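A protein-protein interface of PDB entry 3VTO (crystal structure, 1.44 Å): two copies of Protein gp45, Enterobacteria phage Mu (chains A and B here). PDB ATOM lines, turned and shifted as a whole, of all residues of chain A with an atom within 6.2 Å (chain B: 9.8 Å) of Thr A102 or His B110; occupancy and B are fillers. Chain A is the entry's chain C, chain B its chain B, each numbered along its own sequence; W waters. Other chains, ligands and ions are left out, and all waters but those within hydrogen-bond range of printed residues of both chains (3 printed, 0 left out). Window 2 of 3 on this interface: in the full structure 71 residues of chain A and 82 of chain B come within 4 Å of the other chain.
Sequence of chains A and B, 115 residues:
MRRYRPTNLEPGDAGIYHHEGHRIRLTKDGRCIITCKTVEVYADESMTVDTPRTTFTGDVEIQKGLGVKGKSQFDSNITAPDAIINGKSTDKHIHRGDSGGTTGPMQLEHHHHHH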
ATOM      1  N   LYS A  92       8.318  24.809  16.244  1.00  0.00           N
ATOM      2  CA  LYS A  92       9.718  24.951  16.680  1.00  0.00           C
ATOM      3  C   LYS A  92      10.707  24.996  15.526  1.00  0.00           C
ATOM      4  O   LYS A  92      11.926  24.984  15.752  1.00  0.00           O
ATOM      5  CB  LYS A  92      10.073  23.828  17.646  1.00  0.00           C
ATOM      6  CG  LYS A  92       9.187  23.842  18.892  1.00  0.00           C
ATOM      7  CD  LYS A  92       9.633  22.857  19.930  1.00  0.00           C
ATOM      8  CE  LYS A  92       9.675  21.459  19.377  1.00  0.00           C
ATOM      9  NZ  LYS A  92       8.320  20.907  19.321  1.00  0.00           N
ATOM     10  N   ILE A  94      13.161  25.951  12.396  1.00  0.00           N
ATOM     11  CA  ILE A  94      14.170  26.960  12.179  1.00  0.00           C
ATOM     12  C   ILE A  94      14.528  26.994  10.689  1.00  0.00           C
ATOM     13  O   ILE A  94      14.004  26.198   9.883  1.00  0.00           O
ATOM     14  CB  ILE A  94      15.423  26.669  12.986  1.00  0.00           C
ATOM     15  CG1 ILE A  94      16.108  25.338  12.568  1.00  0.00           C
ATOM     16  CG2 ILE A  94      15.063  26.761  14.467  1.00  0.00           C
ATOM     17  CD1 ILE A  94      17.360  24.954  13.387  1.00  0.00           C
ATOM     18  N   HIS A  95      15.457  27.876  10.335  1.00  0.00           N
ATOM     19  CA  HIS A  95      16.005  27.921   8.966  1.00  0.00           C
ATOM     20  C   HIS A  95      17.521  28.164   9.025  1.00  0.00           C
ATOM     21  O   HIS A  95      18.006  28.723  10.027  1.00  0.00           O
ATOM     22  CB  HIS A  95      15.398  29.081   8.152  1.00  0.00           C
ATOM     23  CG  HIS A  95      13.903  29.045   8.078  1.00  0.00           C
ATOM     24  ND1 HIS A  95      13.212  28.629   6.954  1.00  0.00           N
ATOM     25  CD2 HIS A  95      12.960  29.397   8.983  1.00  0.00           C
ATOM     26  CE1 HIS A  95      11.903  28.703   7.188  1.00  0.00           C
ATOM     27  NE2 HIS A  95      11.729  29.160   8.420  1.00  0.00           N
ATOM     28  N   ARG A  96      18.236  27.836   7.949  1.00  0.00           N
ATOM     29  CA  ARG A  96      19.583  28.363   7.752  1.00  0.00           C
ATOM     30  C   ARG A  96      19.373  29.845   7.404  1.00  0.00           C
ATOM     31  O   ARG A  96      18.606  30.186   6.473  1.00  0.00           O
ATOM     32  CB  ARG A  96      20.309  27.629   6.613  1.00  0.00           C
ATOM     33  CG  ARG A  96      21.756  28.107   6.422  1.00  0.00           C
ATOM     34  CD  ARG A  96      22.430  27.447   5.193  1.00  0.00           C
ATOM     35  NE  ARG A  96      23.658  28.159   4.799  1.00  0.00           N
ATOM     36  CZ  ARG A  96      24.906  27.868   5.187  1.00  0.00           C
ATOM     37  NH1 ARG A  96      25.143  26.844   6.010  1.00  0.00           N
ATOM     38  NH2 ARG A  96      25.934  28.617   4.749  1.00  0.00           N
ATOM     39  N   GLY A  97      20.011  30.728   8.172  1.00  0.00           N
ATOM     40  CA  GLY A  97      19.838  32.163   7.932  1.00  0.00           C
ATOM     41  C   GLY A  97      20.647  32.685   6.740  1.00  0.00           C
ATOM     42  O   GLY A  97      21.428  31.928   6.125  1.00  0.00           O
ATOM     43  N   GLY A 100      24.455  32.146   6.921  1.00  0.00           N
ATOM     44  CA  GLY A 100      24.933  30.792   7.065  1.00  0.00           C
ATOM     45  C   GLY A 100      24.893  30.198   8.452  1.00  0.00           C
ATOM     46  O   GLY A 100      25.371  29.080   8.636  1.00  0.00           O
ATOM     47  N   GLY A 101      24.283  30.916   9.395  1.00  0.00           N
ATOM     48  CA  GLY A 101      24.013  30.372  10.715  1.00  0.00           C
ATOM     49  C   GLY A 101      22.609  29.793  10.747  1.00  0.00           C
ATOM     50  O   GLY A 101      22.034  29.448   9.728  1.00  0.00           O
ATOM     51  N   THR A 102      22.056  29.673  11.932  1.00  0.00           N
ATOM     52  CA  THR A 102      20.687  29.238  12.070  1.00  0.00           C
ATOM     53  C   THR A 102      19.836  30.310  12.716  1.00  0.00           C
ATOM     54  O   THR A 102      20.317  31.066  13.583  1.00  0.00           O
ATOM     55  CB  THR A 102      20.560  27.931  12.811  1.00  0.00           C
ATOM     56  OG1 THR A 102      21.168  28.042  14.108  1.00  0.00           O
ATOM     57  CG2 THR A 102      21.200  26.830  11.972  1.00  0.00           C
ATOM     58  N   THR A 103      18.581  30.381  12.270  1.00  0.00           N
ATOM     59  CA  THR A 103      17.623  31.246  12.895  1.00  0.00           C
ATOM     60  C   THR A 103      17.169  30.623  14.215  1.00  0.00           C
ATOM     61  O   THR A 103      17.366  29.418  14.464  1.00  0.00           O
ATOM     62  CB  THR A 103      16.392  31.500  12.024  1.00  0.00           C
ATOM     63  OG1 THR A 103      15.605  30.309  11.938  1.00  0.00           O
ATOM     64  CG2 THR A 103      16.791  31.969  10.644  1.00  0.00           C
ATOM     65  N   GLY A 104      16.466  31.432  14.993  1.00  0.00           N
ATOM     66  CA  GLY A 104      15.668  30.899  16.086  1.00  0.00           C
ATOM     67  C   GLY A 104      14.365  30.263  15.604  1.00  0.00           C
ATOM     68  O   GLY A 104      14.044  30.255  14.380  1.00  0.00           O
ATOM     69  N   GLY B  97      16.047  37.230   5.291  1.00  0.00           N
ATOM     70  CA  GLY B  97      16.889  37.126   6.490  1.00  0.00           C
ATOM     71  C   GLY B  97      17.106  38.452   7.177  1.00  0.00           C
ATOM     72  O   GLY B  97      16.603  39.503   6.717  1.00  0.00           O
ATOM     73  N   ASP B  98      17.821  38.419   8.307  1.00  0.00           N
ATOM     74  CA  ASP B  98      18.051  39.636   9.042  1.00  0.00           C
ATOM     75  C   ASP B  98      19.191  40.473   8.525  1.00  0.00           C
ATOM     76  O   ASP B  98      19.463  41.529   9.099  1.00  0.00           O
ATOM     77  CB  ASP B  98      18.180  39.365  10.569  1.00  0.00           C
ATOM     78  CG  ASP B  98      19.419  38.560  10.937  1.00  0.00           C
ATOM     79  OD1 ASP B  98      20.251  38.238  10.059  1.00  0.00           O
ATOM     80  OD2 ASP B  98      19.592  38.280  12.151  1.00  0.00           O
ATOM     81  N   THR B 103      16.707  33.379   3.796  1.00  0.00           N
ATOM     82  CA  THR B 103      17.011  32.162   4.531  1.00  0.00           C
ATOM     83  C   THR B 103      16.830  30.945   3.626  1.00  0.00           C
ATOM     84  O   THR B 103      16.270  31.068   2.509  1.00  0.00           O
ATOM     85  CB  THR B 103      16.062  31.971   5.752  1.00  0.00           C
ATOM     86  OG1 THR B 103      14.754  31.565   5.280  1.00  0.00           O
ATOM     87  CG2 THR B 103      15.962  33.213   6.594  1.00  0.00           C
ATOM     88  N   GLY B 104      17.316  29.789   4.070  1.00  0.00           N
ATOM     89  CA  GLY B 104      16.943  28.506   3.454  1.00  0.00           C
ATOM     90  C   GLY B 104      15.548  28.068   3.856  1.00  0.00           C
ATOM     91  O   GLY B 104      14.840  28.762   4.605  1.00  0.00           O
ATOM     92  N   PRO B 105      15.140  26.890   3.387  1.00  0.00           N
ATOM     93  CA  PRO B 105      13.785  26.359   3.671  1.00  0.00           C
ATOM     94  C   PRO B 105      13.635  25.839   5.095  1.00  0.00           C
ATOM     95  O   PRO B 105      14.618  25.582   5.804  1.00  0.00           O
ATOM     96  CB  PRO B 105      13.662  25.191   2.698  1.00  0.00           C
ATOM     97  CG  PRO B 105      15.105  24.754   2.472  1.00  0.00           C
ATOM     98  CD  PRO B 105      15.931  26.020   2.506  1.00  0.00           C
ATOM     99  N   GLN B 107      13.433  23.904   8.374  1.00  0.00           N
ATOM    100  CA  GLN B 107      14.256  22.812   8.854  1.00  0.00           C
ATOM    101  C   GLN B 107      13.731  22.318  10.161  1.00  0.00           C
ATOM    102  O   GLN B 107      13.071  23.066  10.898  1.00  0.00           O
ATOM    103  CB  GLN B 107      15.690  23.275   9.102  1.00  0.00           C
ATOM    104  CG  GLN B 107      16.494  23.482   7.892  1.00  0.00           C
ATOM    105  CD  GLN B 107      17.939  23.912   8.246  1.00  0.00           C
ATOM    106  OE1 GLN B 107      18.261  24.182   9.395  1.00  0.00           O
ATOM    107  NE2 GLN B 107      18.778  23.957   7.266  1.00  0.00           N
ATOM    108  N   LEU B 108      14.053  21.063  10.432  1.00  0.00           N
ATOM    109  CA  LEU B 108      13.746  20.409  11.675  1.00  0.00           C
ATOM    110  C   LEU B 108      14.169  21.269  12.836  1.00  0.00           C
ATOM    111  O   LEU B 108      15.230  21.876  12.813  1.00  0.00           O
ATOM    112  CB  LEU B 108      14.489  19.068  11.726  1.00  0.00           C
ATOM    113  CG  LEU B 108      14.126  18.098  12.852  1.00  0.00           C
ATOM    114  CD1 LEU B 108      12.710  17.595  12.671  1.00  0.00           C
ATOM    115  CD2 LEU B 108      15.124  16.927  12.945  1.00  0.00           C
ATOM    116  N   GLU B 109      13.323  21.301  13.858  1.00  0.00           N
ATOM    117  CA  GLU B 109      13.654  21.936  15.133  1.00  0.00           C
ATOM    118  C   GLU B 109      14.971  21.414  15.715  1.00  0.00           C
ATOM    119  O   GLU B 109      15.382  20.284  15.443  1.00  0.00           O
ATOM    120  CB  GLU B 109      12.501  21.714  16.127  1.00  0.00           C
ATOM    121  CG  GLU B 109      12.172  20.242  16.508  1.00  0.00           C
ATOM    122  CD  GLU B 109      11.244  19.507  15.522  1.00  0.00           C
ATOM    123  OE1 GLU B 109      11.020  19.967  14.374  1.00  0.00           O
ATOM    124  OE2 GLU B 109      10.756  18.429  15.913  1.00  0.00           O
ATOM    125  N   HIS B 110      15.617  22.268  16.515  1.00  0.00           N
ATOM    126  CA  HIS B 110      16.745  21.864  17.347  1.00  0.00           C
ATOM    127  C   HIS B 110      16.265  20.863  18.398  1.00  0.00           C
ATOM    128  O   HIS B 110      17.068  20.164  19.033  1.00  0.00           O
ATOM    129  CB  HIS B 110      17.347  23.084  18.039  1.00  0.00           C
ATOM    130  CG  HIS B 110      18.364  23.807  17.215  1.00  0.00           C
ATOM    131  ND1 HIS B 110      19.244  23.160  16.371  1.00  0.00           N
ATOM    132  CD2 HIS B 110      18.666  25.127  17.130  1.00  0.00           C
ATOM    133  CE1 HIS B 110      20.031  24.049  15.787  1.00  0.00           C
ATOM    134  NE2 HIS B 110      19.706  25.251  16.237  1.00  0.00           N
HETATM  135  O   HOH W   1      17.928  27.806  16.640  1.00  0.00           O
HETATM  136  O   HOH W   2      17.269  26.251   5.813  1.00  0.00           O
HETATM  137  O   HOH W   3      13.999  24.740  17.460  1.00  0.00           O
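The backbone carbonyl oxygen (O) of Gly B104 sits at hydrogen-bond distance from a ring nitrogen (ND1) of His A95, 2.9 Å away. N of Gly B104 sits at hydrogen-bond distance from O of Arg A96 (2.8 Å). The backbone carbonyl oxygen (O) of Ile A94 lies within hydrogen-bond range of the backbone NH (N) of Gln B107 (2.8 Å).
O of His A95 is in hydrogen-bond range of N of Thr A103 (2.8 Å). The guanidinium group (NH1) of Arg A96 is in hydrogen-bond range of the backbone carbonyl oxygen (O) of Gly A100 (3.5 Å).
Lys A92 touches Glu B109 (O to CB, 3.3 Å). Leu B108 touches Ile A94 (O to CG1, 3.6 Å). Ile A94 touches His B110 (CD1 to CE1, 3.7 Å). Thr B103 touches His A95 (OG1 to ND1, 3.7 Å). His A95 touches Pro B105 (ND1 to C, 3.4 Å). Arg A96 touches Thr B103. OE1 of Gln B107 touches N of Arg A96, 3.9 Å away. Thr A102 touches His B110.
Thr A102 touches just one residue of chain B: His B110 (3.8 Å). Of chain A, only Ile A94 and Thr A102 come within 4 Å of His B110. No residue of chain B comes within 4 Å of Gly A101. Of the printed residues of chain B, Lys A92 touches Glu B109 (3.3 Å). Of the printed residues of chain B, Arg A96 touches Thr B103 (3.2 Å), Gly B104 (2.8 Å) and Gln B107 (3.9 Å). Of the printed residues of chain B, His A95 touches Thr B103 (3.7 Å), Gly B104 (2.9 Å) and Pro B105 (3.4 Å). Printed residues of chain A within 4 Å of Leu B108: Ile A94 (3.6 Å). Of the printed residues of chain A, Glu B109 touches Lys A92 (3.3 Å). The nearest printed residue of chain B that does not touch His A95 is Gln B107 (4.1 Å).
Of the 9 printed residues of chain B, 7 touch a printed residue of chain A. Among the printed residues, no Asp or Glu carboxylate lies within 4 Å of a Lys or Arg side-chain nitrogen of the other chain.
Positions printed for both chains: 97, 103 and 104.
Water W3 bridges O of Lys A92 (2.7 Å) and N of His B110 (3.1 Å). Water W2 lies within hydrogen-bond range of the backbone carbonyl oxygen (O) of Pro B105 (2.7 Å), the backbone NH (N) of Arg A96 (2.8 Å) and the side-chain amide nitrogen (NE2) of Gln B107 (3.1 Å). Water W1 bridges the backbone carbonyl oxygen (O) of Thr A103 and a ring nitrogen (NE2) of His B110.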
